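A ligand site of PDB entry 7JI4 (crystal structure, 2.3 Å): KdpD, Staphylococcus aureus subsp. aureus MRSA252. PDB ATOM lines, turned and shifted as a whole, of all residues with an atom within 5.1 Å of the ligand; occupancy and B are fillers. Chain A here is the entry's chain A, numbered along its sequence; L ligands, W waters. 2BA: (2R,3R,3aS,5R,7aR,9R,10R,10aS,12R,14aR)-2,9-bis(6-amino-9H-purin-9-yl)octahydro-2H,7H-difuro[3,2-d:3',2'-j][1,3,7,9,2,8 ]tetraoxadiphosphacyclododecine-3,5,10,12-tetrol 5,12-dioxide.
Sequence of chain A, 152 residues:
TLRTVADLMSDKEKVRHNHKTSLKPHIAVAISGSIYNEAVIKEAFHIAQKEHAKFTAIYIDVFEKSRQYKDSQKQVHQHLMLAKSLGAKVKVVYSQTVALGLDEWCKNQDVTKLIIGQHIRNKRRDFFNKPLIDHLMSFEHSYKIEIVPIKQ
Water W1 lies within hydrogen-bond range of O2P of the ligand, N of Leu 132 and N of Ile 133.
Water W6 lies within hydrogen-bond range of O1P of the ligand (2.7 Å) and OH of Tyr 69 (3.2 Å).
Water W7 bridges an oxygen (O2P1) of the ligand and the backbone carbonyl oxygen (O) of Gln 118.
Water W9 lies within hydrogen-bond range of an oxygen (O1P) of the ligand (2.7 Å) and the backbone carbonyl oxygen of Lys 130 (2.7 Å).
Water W3 bridges O2'1 of the ligand (2.8 Å) and NE2 of His 119 (3.3 Å).
Water W2 bridges N61 of the ligand (3.0 Å) and N of Gly 33 (3.1 Å).
The backbone carbonyl oxygen (O) of Ile 31 sits close to a nitrogen (N3) of the ligand (3.1 Å).
The backbone NH (N) of Gly 33 sits close to a nitrogen (N61) of the ligand (3.5 Å).
The side-chain hydroxyl (OH) of Tyr 69 sits close to a nitrogen (N91) of the ligand.
Merely in contact with the ligand: His 119 (3.3 Å), Ile 116 (3.4 Å), Val 98 (3.4 Å), Ile 58 (3.5 Å), Tyr 36 (3.5 Å), Asn 37 (3.6 Å), Pro 131 (3.6 Å), Tyr 59 (3.7 Å), Gln 118 (3.8 Å) and Val 40 (3.8 Å).
19 residues have an atom within 4 Å of the ligand: Ala 30, Ile 31, Ser 32, Gly 33, Ser 34, Tyr 36, Asn 37, Val 40, Ile 58, Tyr 59, Ile 60, Tyr 69, Val 98, Ile 116, Gly 117, Gln 118, His 119, Pro 131 and Leu 132.
The nearest printed residue that does not touch the ligand is Leu 102 (4.2 Å).
The side-chain hydroxyl (OG) of Ser 34 sits at hydrogen-bond distance from an oxygen (O1P1) of the ligand (2.7 Å).
O2P of the ligand sits at hydrogen-bond distance from N of Leu 132 (2.9 Å).
A nitrogen (N6) of the ligand lies within hydrogen-bond range of the backbone carbonyl oxygen of Ile 60, at 2.8 Å.
An oxygen (O2') of the ligand sits at hydrogen-bond distance from the backbone carbonyl oxygen (O) of Ala 30 (2.6 Å).
An oxygen (O1P1) of the ligand is in hydrogen-bond range of the side-chain hydroxyl (OG) of Ser 32 (2.5 Å).
The backbone NH (N) of Gly 117 is in hydrogen-bond range of an oxygen (O3') of the ligand (2.9 Å).
The backbone NH of Ile 60 lies within hydrogen-bond range of a nitrogen (N1) of the ligand, at 2.9 Å.
OG of Ser 34 sits at hydrogen-bond distance from N of Asn 37, at 3.3 Å.
The side-chain amide nitrogen of Asn 37 is in hydrogen-bond range of the backbone carbonyl oxygen of Ala 30 (3.1 Å).
OG of Ser 32 sits at hydrogen-bond distance from OG of Ser 34, 2.9 Å away.
The backbone NH of Ala 30 sits at hydrogen-bond distance from the backbone carbonyl oxygen of Ile 115 (2.9 Å).
The backbone NH (N) of Ser 32 lies within hydrogen-bond range of the side-chain amide oxygen (OD1) of Asn 37, at 3.0 Å.
The backbone carbonyl oxygen (O) of Ile 58 sits at hydrogen-bond distance from the backbone NH (N) of Ile 31 (2.8 Å).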
ATOM      1  N   ALA A  30     -20.111 -21.217 -23.975  1.00  0.00           N
ATOM      2  CA  ALA A  30     -20.666 -19.994 -23.412  1.00  0.00           C
ATOM      3  C   ALA A  30     -19.514 -19.238 -22.760  1.00  0.00           C
ATOM      4  O   ALA A  30     -18.939 -19.708 -21.762  1.00  0.00           O
ATOM      5  CB  ALA A  30     -21.767 -20.313 -22.410  1.00  0.00           C
ATOM      6  N   ILE A  31     -19.190 -18.065 -23.319  1.00  0.00           N
ATOM      7  CA  ILE A  31     -18.026 -17.272 -22.935  1.00  0.00           C
ATOM      8  C   ILE A  31     -18.386 -16.375 -21.763  1.00  0.00           C
ATOM      9  O   ILE A  31     -19.448 -15.735 -21.751  1.00  0.00           O
ATOM     10  CB  ILE A  31     -17.556 -16.407 -24.112  1.00  0.00           C
ATOM     11  CG1 ILE A  31     -17.386 -17.272 -25.353  1.00  0.00           C
ATOM     12  CG2 ILE A  31     -16.277 -15.666 -23.755  1.00  0.00           C
ATOM     13  CD1 ILE A  31     -16.122 -18.002 -25.339  1.00  0.00           C
ATOM     14  N   SER A  32     -17.478 -16.266 -20.796  1.00  0.00           N
ATOM     15  CA  SER A  32     -17.616 -15.238 -19.779  1.00  0.00           C
ATOM     16  C   SER A  32     -16.242 -14.645 -19.498  1.00  0.00           C
ATOM     17  O   SER A  32     -15.222 -15.095 -20.033  1.00  0.00           O
ATOM     18  CB  SER A  32     -18.241 -15.778 -18.497  1.00  0.00           C
ATOM     19  OG  SER A  32     -17.245 -16.161 -17.572  1.00  0.00           O
ATOM     20  N   GLY A  33     -16.225 -13.617 -18.662  1.00  0.00           N
ATOM     21  CA  GLY A  33     -15.002 -12.996 -18.225  1.00  0.00           C
ATOM     22  C   GLY A  33     -14.339 -13.657 -17.030  1.00  0.00           C
ATOM     23  O   GLY A  33     -13.359 -13.110 -16.512  1.00  0.00           O
ATOM     24  N   SER A  34     -14.833 -14.794 -16.567  1.00  0.00           N
ATOM     25  CA  SER A  34     -14.178 -15.462 -15.448  1.00  0.00           C
ATOM     26  C   SER A  34     -12.821 -16.004 -15.867  1.00  0.00           C
ATOM     27  O   SER A  34     -12.591 -16.327 -17.034  1.00  0.00           O
ATOM     28  CB  SER A  34     -15.019 -16.629 -14.923  1.00  0.00           C
ATOM     29  OG  SER A  34     -15.212 -17.506 -15.982  1.00  0.00           O
ATOM     30  N   TYR A  36     -11.831 -18.861 -15.041  1.00  0.00           N
ATOM     31  CA  TYR A  36     -12.100 -20.274 -15.351  1.00  0.00           C
ATOM     32  C   TYR A  36     -12.561 -20.513 -16.776  1.00  0.00           C
ATOM     33  O   TYR A  36     -12.562 -21.664 -17.211  1.00  0.00           O
ATOM     34  CB  TYR A  36     -13.173 -20.854 -14.424  1.00  0.00           C
ATOM     35  CG  TYR A  36     -12.964 -20.579 -12.970  1.00  0.00           C
ATOM     36  CD1 TYR A  36     -11.859 -21.111 -12.301  1.00  0.00           C
ATOM     37  CD2 TYR A  36     -13.839 -19.777 -12.252  1.00  0.00           C
ATOM     38  CE1 TYR A  36     -11.645 -20.862 -10.950  1.00  0.00           C
ATOM     39  CE2 TYR A  36     -13.644 -19.519 -10.909  1.00  0.00           C
ATOM     40  CZ  TYR A  36     -12.547 -20.062 -10.258  1.00  0.00           C
ATOM     41  OH  TYR A  36     -12.351 -19.804  -8.915  1.00  0.00           O
ATOM     42  N   ASN A  37     -13.015 -19.486 -17.490  1.00  0.00           N
ATOM     43  CA  ASN A  37     -13.654 -19.727 -18.777  1.00  0.00           C
ATOM     44  C   ASN A  37     -12.660 -20.225 -19.819  1.00  0.00           C
ATOM     45  O   ASN A  37     -13.041 -20.967 -20.741  1.00  0.00           O
ATOM     46  CB  ASN A  37     -14.351 -18.457 -19.265  1.00  0.00           C
ATOM     47  CG  ASN A  37     -15.287 -18.704 -20.417  1.00  0.00           C
ATOM     48  OD1 ASN A  37     -15.148 -18.089 -21.470  1.00  0.00           O
ATOM     49  ND2 ASN A  37     -16.240 -19.616 -20.244  1.00  0.00           N
ATOM     50  N   VAL A  40     -12.659 -23.782 -20.028  1.00  0.00           N
ATOM     51  CA  VAL A  40     -13.905 -24.230 -20.637  1.00  0.00           C
ATOM     52  C   VAL A  40     -13.803 -24.141 -22.163  1.00  0.00           C
ATOM     53  O   VAL A  40     -14.329 -25.012 -22.881  1.00  0.00           O
ATOM     54  CB  VAL A  40     -15.096 -23.422 -20.093  1.00  0.00           C
ATOM     55  CG1 VAL A  40     -16.436 -24.001 -20.631  1.00  0.00           C
ATOM     56  CG2 VAL A  40     -15.058 -23.400 -18.567  1.00  0.00           C
ATOM     57  N   ILE A  58     -20.240 -18.072 -27.758  1.00  0.00           N
ATOM     58  CA  ILE A  58     -21.311 -17.108 -27.572  1.00  0.00           C
ATOM     59  C   ILE A  58     -21.057 -16.410 -26.239  1.00  0.00           C
ATOM     60  O   ILE A  58     -20.934 -17.064 -25.196  1.00  0.00           O
ATOM     61  CB  ILE A  58     -22.691 -17.782 -27.612  1.00  0.00           C
ATOM     62  CG1 ILE A  58     -23.823 -16.758 -27.709  1.00  0.00           C
ATOM     63  CG2 ILE A  58     -22.911 -18.649 -26.373  1.00  0.00           C
ATOM     64  CD1 ILE A  58     -23.783 -15.903 -28.938  1.00  0.00           C
ATOM     65  N   TYR A  59     -20.931 -15.088 -26.290  1.00  0.00           N
ATOM     66  CA  TYR A  59     -20.916 -14.243 -25.104  1.00  0.00           C
ATOM     67  C   TYR A  59     -22.179 -13.386 -25.087  1.00  0.00           C
ATOM     68  O   TYR A  59     -22.531 -12.768 -26.089  1.00  0.00           O
ATOM     69  CB  TYR A  59     -19.676 -13.338 -25.111  1.00  0.00           C
ATOM     70  CG  TYR A  59     -19.691 -12.275 -24.052  1.00  0.00           C
ATOM     71  CD1 TYR A  59     -19.587 -12.606 -22.692  1.00  0.00           C
ATOM     72  CD2 TYR A  59     -19.820 -10.930 -24.388  1.00  0.00           C
ATOM     73  CE1 TYR A  59     -19.598 -11.621 -21.718  1.00  0.00           C
ATOM     74  CE2 TYR A  59     -19.836  -9.940 -23.420  1.00  0.00           C
ATOM     75  CZ  TYR A  59     -19.709 -10.280 -22.086  1.00  0.00           C
ATOM     76  OH  TYR A  59     -19.754  -9.291 -21.127  1.00  0.00           O
ATOM     77  N   ILE A  60     -22.878 -13.375 -23.955  1.00  0.00           N
ATOM     78  CA  ILE A  60     -24.056 -12.535 -23.759  1.00  0.00           C
ATOM     79  C   ILE A  60     -23.594 -11.284 -23.021  1.00  0.00           C
ATOM     80  O   ILE A  60     -23.083 -11.352 -21.894  1.00  0.00           O
ATOM     81  CB  ILE A  60     -25.178 -13.264 -22.996  1.00  0.00           C
ATOM     82  CG1 ILE A  60     -25.446 -14.637 -23.592  1.00  0.00           C
ATOM     83  CG2 ILE A  60     -26.490 -12.500 -23.080  1.00  0.00           C
ATOM     84  CD1 ILE A  60     -25.925 -14.605 -25.064  1.00  0.00           C
ATOM     85  N   ASP A  61     -23.728 -10.129 -23.664  1.00  0.00           N
ATOM     86  CA  ASP A  61     -23.370  -8.856 -23.055  1.00  0.00           C
ATOM     87  C   ASP A  61     -24.587  -8.272 -22.360  1.00  0.00           C
ATOM     88  O   ASP A  61     -25.621  -8.012 -22.994  1.00  0.00           O
ATOM     89  CB  ASP A  61     -22.808  -7.893 -24.097  1.00  0.00           C
ATOM     90  CG  ASP A  61     -22.095  -6.713 -23.463  1.00  0.00           C
ATOM     91  OD1 ASP A  61     -22.675  -6.118 -22.525  1.00  0.00           O
ATOM     92  OD2 ASP A  61     -20.956  -6.383 -23.890  1.00  0.00           O
ATOM     93  N   TYR A  69     -18.655  -7.070 -12.200  1.00  0.00           N
ATOM     94  CA  TYR A  69     -17.392  -7.635 -12.687  1.00  0.00           C
ATOM     95  C   TYR A  69     -16.570  -6.548 -13.356  1.00  0.00           C
ATOM     96  O   TYR A  69     -16.214  -6.624 -14.535  1.00  0.00           O
ATOM     97  CB  TYR A  69     -17.614  -8.799 -13.646  1.00  0.00           C
ATOM     98  CG  TYR A  69     -18.375  -9.996 -13.116  1.00  0.00           C
ATOM     99  CD1 TYR A  69     -17.884 -10.756 -12.053  1.00  0.00           C
ATOM    100  CD2 TYR A  69     -19.577 -10.388 -13.710  1.00  0.00           C
ATOM    101  CE1 TYR A  69     -18.578 -11.866 -11.578  1.00  0.00           C
ATOM    102  CE2 TYR A  69     -20.282 -11.487 -13.248  1.00  0.00           C
ATOM    103  CZ  TYR A  69     -19.794 -12.225 -12.180  1.00  0.00           C
ATOM    104  OH  TYR A  69     -20.520 -13.330 -11.738  1.00  0.00           O
ATOM    105  N   SER A  72     -13.837  -6.414 -16.729  1.00  0.00           N
ATOM    106  CA  SER A  72     -13.617  -7.735 -17.297  1.00  0.00           C
ATOM    107  C   SER A  72     -13.774  -7.729 -18.814  1.00  0.00           C
ATOM    108  O   SER A  72     -13.680  -8.801 -19.439  1.00  0.00           O
ATOM    109  CB  SER A  72     -14.578  -8.760 -16.680  1.00  0.00           C
ATOM    110  N   VAL A  98     -28.265 -12.873 -19.134  1.00  0.00           N
ATOM    111  CA  VAL A  98     -27.453 -13.965 -19.651  1.00  0.00           C
ATOM    112  C   VAL A  98     -28.338 -15.141 -20.072  1.00  0.00           C
ATOM    113  O   VAL A  98     -28.214 -15.650 -21.191  1.00  0.00           O
ATOM    114  CB  VAL A  98     -26.401 -14.401 -18.631  1.00  0.00           C
ATOM    115  CG1 VAL A  98     -25.617 -15.570 -19.207  1.00  0.00           C
ATOM    116  CG2 VAL A  98     -25.446 -13.245 -18.342  1.00  0.00           C
ATOM    117  N   LEU A 102     -28.686 -16.465 -23.974  1.00  0.00           N
ATOM    118  CA  LEU A 102     -28.202 -17.790 -24.356  1.00  0.00           C
ATOM    119  C   LEU A 102     -29.316 -18.674 -24.870  1.00  0.00           C
ATOM    120  O   LEU A 102     -29.176 -19.334 -25.901  1.00  0.00           O
ATOM    121  CB  LEU A 102     -27.549 -18.461 -23.162  1.00  0.00           C
ATOM    122  CG  LEU A 102     -26.079 -18.252 -22.869  1.00  0.00           C
ATOM    123  CD1 LEU A 102     -25.677 -19.234 -21.802  1.00  0.00           C
ATOM    124  CD2 LEU A 102     -25.254 -18.428 -24.132  1.00  0.00           C
ATOM    125  N   ILE A 115     -21.847 -25.779 -23.996  1.00  0.00           N
ATOM    126  CA  ILE A 115     -20.800 -26.095 -23.039  1.00  0.00           C
ATOM    127  C   ILE A 115     -20.577 -24.877 -22.157  1.00  0.00           C
ATOM    128  O   ILE A 115     -20.303 -23.779 -22.649  1.00  0.00           O
ATOM    129  CB  ILE A 115     -19.509 -26.522 -23.766  1.00  0.00           C
ATOM    130  CG1 ILE A 115     -19.796 -27.815 -24.524  1.00  0.00           C
ATOM    131  CG2 ILE A 115     -18.378 -26.695 -22.770  1.00  0.00           C
ATOM    132  CD1 ILE A 115     -18.662 -28.268 -25.348  1.00  0.00           C
ATOM    133  N   ILE A 116     -20.725 -25.074 -20.853  1.00  0.00           N
ATOM    134  CA  ILE A 116     -20.654 -23.980 -19.897  1.00  0.00           C
ATOM    135  C   ILE A 116     -19.736 -24.430 -18.769  1.00  0.00           C
ATOM    136  O   ILE A 116     -19.499 -25.622 -18.572  1.00  0.00           O
ATOM    137  CB  ILE A 116     -22.040 -23.568 -19.336  1.00  0.00           C
ATOM    138  CG1 ILE A 116     -22.532 -24.587 -18.319  1.00  0.00           C
ATOM    139  CG2 ILE A 116     -23.061 -23.424 -20.459  1.00  0.00           C
ATOM    140  CD1 ILE A 116     -23.844 -24.207 -17.645  1.00  0.00           C
ATOM    141  N   GLY A 117     -19.220 -23.450 -18.027  1.00  0.00           N
ATOM    142  CA  GLY A 117     -18.414 -23.752 -16.870  1.00  0.00           C
ATOM    143  C   GLY A 117     -19.236 -23.957 -15.610  1.00  0.00           C
ATOM    144  O   GLY A 117     -20.418 -23.623 -15.519  1.00  0.00           O
ATOM    145  N   GLN A 118     -18.558 -24.539 -14.620  1.00  0.00           N
ATOM    146  CA  GLN A 118     -19.141 -24.794 -13.315  1.00  0.00           C
ATOM    147  C   GLN A 118     -19.415 -23.492 -12.584  1.00  0.00           C
ATOM    148  O   GLN A 118     -18.548 -22.622 -12.497  1.00  0.00           O
ATOM    149  CB  GLN A 118     -18.183 -25.657 -12.505  1.00  0.00           C
ATOM    150  CG  GLN A 118     -18.688 -26.110 -11.184  1.00  0.00           C
ATOM    151  CD  GLN A 118     -17.809 -27.217 -10.624  1.00  0.00           C
ATOM    152  OE1 GLN A 118     -16.589 -27.074 -10.542  1.00  0.00           O
ATOM    153  NE2 GLN A 118     -18.423 -28.349 -10.261  1.00  0.00           N
ATOM    154  N   HIS A 119     -20.620 -23.356 -12.046  1.00  0.00           N
ATOM    155  CA  HIS A 119     -20.876 -22.297 -11.078  1.00  0.00           C
ATOM    156  C   HIS A 119     -20.310 -22.725  -9.733  1.00  0.00           C
ATOM    157  O   HIS A 119     -20.485 -23.875  -9.316  1.00  0.00           O
ATOM    158  CB  HIS A 119     -22.373 -22.032 -10.966  1.00  0.00           C
ATOM    159  CG  HIS A 119     -22.748 -21.064  -9.874  1.00  0.00           C
ATOM    160  ND1 HIS A 119     -23.089 -21.476  -8.600  1.00  0.00           N
ATOM    161  CD2 HIS A 119     -22.862 -19.708  -9.877  1.00  0.00           C
ATOM    162  CE1 HIS A 119     -23.398 -20.418  -7.864  1.00  0.00           C
ATOM    163  NE2 HIS A 119     -23.269 -19.339  -8.609  1.00  0.00           N
ATOM    164  N   ILE A 120     -19.648 -21.805  -9.049  1.00  0.00           N
ATOM    165  CA  ILE A 120     -19.258 -22.013  -7.656  1.00  0.00           C
ATOM    166  C   ILE A 120     -19.989 -20.986  -6.785  1.00  0.00           C
ATOM    167  O   ILE A 120     -20.011 -19.787  -7.098  1.00  0.00           O
ATOM    168  CB  ILE A 120     -17.730 -21.971  -7.473  1.00  0.00           C
ATOM    169  CG1 ILE A 120     -17.359 -22.440  -6.056  1.00  0.00           C
ATOM    170  CG2 ILE A 120     -17.113 -20.604  -7.838  1.00  0.00           C
ATOM    171  CD1 ILE A 120     -18.122 -23.670  -5.584  1.00  0.00           C
ATOM    172  N   LYS A 130     -28.129 -16.478  -8.942  1.00  0.00           N
ATOM    173  CA  LYS A 130     -28.280 -17.917  -9.000  1.00  0.00           C
ATOM    174  C   LYS A 130     -27.372 -18.485 -10.094  1.00  0.00           C
ATOM    175  O   LYS A 130     -26.977 -17.764 -11.013  1.00  0.00           O
ATOM    176  CB  LYS A 130     -29.729 -18.296  -9.284  1.00  0.00           C
ATOM    177  CG  LYS A 130     -30.712 -17.873  -8.192  1.00  0.00           C
ATOM    178  CD  LYS A 130     -32.141 -18.123  -8.613  1.00  0.00           C
ATOM    179  CE  LYS A 130     -32.372 -19.600  -8.823  1.00  0.00           C
ATOM    180  NZ  LYS A 130     -33.805 -19.929  -9.079  1.00  0.00           N
ATOM    181  N   PRO A 131     -27.027 -19.766 -10.011  1.00  0.00           N
ATOM    182  CA  PRO A 131     -26.282 -20.393 -11.104  1.00  0.00           C
ATOM    183  C   PRO A 131     -27.039 -20.257 -12.424  1.00  0.00           C
ATOM    184  O   PRO A 131     -28.263 -20.399 -12.471  1.00  0.00           O
ATOM    185  CB  PRO A 131     -26.175 -21.862 -10.674  1.00  0.00           C
ATOM    186  CG  PRO A 131     -26.393 -21.862  -9.210  1.00  0.00           C
ATOM    187  CD  PRO A 131     -27.289 -20.711  -8.913  1.00  0.00           C
ATOM    188  N   LEU A 132     -26.286 -19.977 -13.491  1.00  0.00           N
ATOM    189  CA  LEU A 132     -26.903 -19.841 -14.812  1.00  0.00           C
ATOM    190  C   LEU A 132     -27.747 -21.064 -15.122  1.00  0.00           C
ATOM    191  O   LEU A 132     -28.823 -20.945 -15.721  1.00  0.00           O
ATOM    192  CB  LEU A 132     -25.826 -19.643 -15.881  1.00  0.00           C
ATOM    193  CG  LEU A 132     -26.268 -19.929 -17.314  1.00  0.00           C
ATOM    194  CD1 LEU A 132     -27.486 -19.086 -17.710  1.00  0.00           C
ATOM    195  CD2 LEU A 132     -25.120 -19.630 -18.263  1.00  0.00           C
ATOM    196  N   ILE A 133     -27.287 -22.226 -14.693  1.00  0.00           N
ATOM    197  CA  ILE A 133     -27.957 -23.470 -15.036  1.00  0.00           C
ATOM    198  C   ILE A 133     -29.358 -23.543 -14.431  1.00  0.00           C
ATOM    199  O   ILE A 133     -30.254 -24.210 -14.993  1.00  0.00           O
ATOM    200  CB  ILE A 133     -27.055 -24.651 -14.587  1.00  0.00           C
ATOM    201  CG1 ILE A 133     -27.574 -25.970 -15.125  1.00  0.00           C
ATOM    202  CG2 ILE A 133     -26.898 -24.665 -13.093  1.00  0.00           C
ATOM    203  CD1 ILE A 133     -27.254 -26.141 -16.584  1.00  0.00           C
HETATM  204  P   2BA L   1     -22.323 -18.952 -13.663  1.00  0.00           P
HETATM  205  O1P 2BA L   1     -22.799 -17.509 -13.645  1.00  0.00           O
HETATM  206  O2P 2BA L   1     -23.455 -19.735 -13.242  1.00  0.00           O
HETATM  207  O5' 2BA L   1     -21.996 -19.341 -15.235  1.00  0.00           O
HETATM  208  C5' 2BA L   1     -21.719 -20.712 -15.463  1.00  0.00           C
HETATM  209  C4' 2BA L   1     -21.284 -20.681 -17.009  1.00  0.00           C
HETATM  210  O4' 2BA L   1     -22.160 -19.947 -17.550  1.00  0.00           O
HETATM  211  C3' 2BA L   1     -19.952 -19.882 -17.223  1.00  0.00           C
HETATM  212  O3' 2BA L   1     -18.858 -20.689 -17.127  1.00  0.00           O
HETATM  213  C2' 2BA L   1     -20.168 -19.514 -18.678  1.00  0.00           C
HETATM  214  O2' 2BA L   1     -19.743 -20.721 -19.478  1.00  0.00           O
HETATM  215  C1' 2BA L   1     -21.452 -19.298 -18.850  1.00  0.00           C
HETATM  216  N9  2BA L   1     -21.677 -17.926 -18.935  1.00  0.00           N
HETATM  217  C8  2BA L   1     -21.619 -17.220 -17.792  1.00  0.00           C
HETATM  218  N7  2BA L   1     -21.835 -15.932 -18.077  1.00  0.00           N
HETATM  219  C5  2BA L   1     -22.019 -15.842 -19.425  1.00  0.00           C
HETATM  220  C6  2BA L   1     -22.274 -14.776 -20.247  1.00  0.00           C
HETATM  221  N6  2BA L   1     -22.424 -13.353 -19.983  1.00  0.00           N
HETATM  222  N1  2BA L   1     -22.423 -14.982 -21.552  1.00  0.00           N
HETATM  223  C2  2BA L   1     -22.333 -16.225 -22.090  1.00  0.00           C
HETATM  224  N3  2BA L   1     -22.066 -17.253 -21.292  1.00  0.00           N
HETATM  225  C4  2BA L   1     -21.924 -17.053 -19.941  1.00  0.00           C
HETATM  226  P1  2BA L   1     -17.561 -19.920 -16.304  1.00  0.00           P
HETATM  227 O1P1 2BA L   1     -17.404 -18.632 -17.001  1.00  0.00           O
HETATM  228 O2P1 2BA L   1     -16.231 -20.633 -16.191  1.00  0.00           O
HETATM  229 O5'1 2BA L   1     -18.388 -19.687 -14.839  1.00  0.00           O
HETATM  230 C5'1 2BA L   1     -17.562 -19.008 -13.907  1.00  0.00           C
HETATM  231 C4'1 2BA L   1     -18.488 -18.830 -12.655  1.00  0.00           C
HETATM  232 O4'1 2BA L   1     -17.865 -17.863 -11.977  1.00  0.00           O
HETATM  233 C3'1 2BA L   1     -19.857 -18.324 -13.079  1.00  0.00           C
HETATM  234 O3'1 2BA L   1     -20.876 -19.155 -12.725  1.00  0.00           O
HETATM  235 C2'1 2BA L   1     -20.031 -17.043 -12.185  1.00  0.00           C
HETATM  236 O2'1 2BA L   1     -20.556 -17.529 -10.830  1.00  0.00           O
HETATM  237 C1'1 2BA L   1     -18.849 -16.590 -12.025  1.00  0.00           C
HETATM  238  N91 2BA L   1     -18.453 -15.587 -13.012  1.00  0.00           N
HETATM  239  C81 2BA L   1     -19.205 -15.358 -14.166  1.00  0.00           C
HETATM  240  N71 2BA L   1     -18.651 -14.373 -14.849  1.00  0.00           N
HETATM  241  C51 2BA L   1     -17.563 -13.967 -14.123  1.00  0.00           C
HETATM  242  C61 2BA L   1     -16.638 -12.993 -14.359  1.00  0.00           C
HETATM  243  N61 2BA L   1     -16.734 -12.195 -15.560  1.00  0.00           N
HETATM  244  N11 2BA L   1     -15.646 -12.793 -13.473  1.00  0.00           N
HETATM  245  C21 2BA L   1     -15.553 -13.552 -12.343  1.00  0.00           C
HETATM  246  N31 2BA L   1     -16.478 -14.527 -12.107  1.00  0.00           N
HETATM  247  C41 2BA L   1     -17.467 -14.719 -13.005  1.00  0.00           C
HETATM  248  O   HOH W   1     -24.190 -22.095 -13.650  1.00  0.00           O
HETATM  249  O   HOH W   2     -18.555 -11.793 -17.866  1.00  0.00           O
HETATM  250  O   HOH W   3     -22.963 -16.389 -10.094  1.00  0.00           O
HETATM  251  O   HOH W   4     -21.344 -12.068 -17.551  1.00  0.00           O
HETATM  252  O   HOH W   5     -12.748 -14.738 -12.499  1.00  0.00           O
HETATM  253  O   HOH W   6     -22.167 -14.908 -13.942  1.00  0.00           O
HETATM  254  O   HOH W   7     -16.091 -22.523 -14.254  1.00  0.00           O
HETATM  255  O   HOH W   8     -22.711 -13.677 -16.121  1.00  0.00           O
HETATM  256  O   HOH W   9     -24.712 -16.557 -11.976  1.00  0.00           O
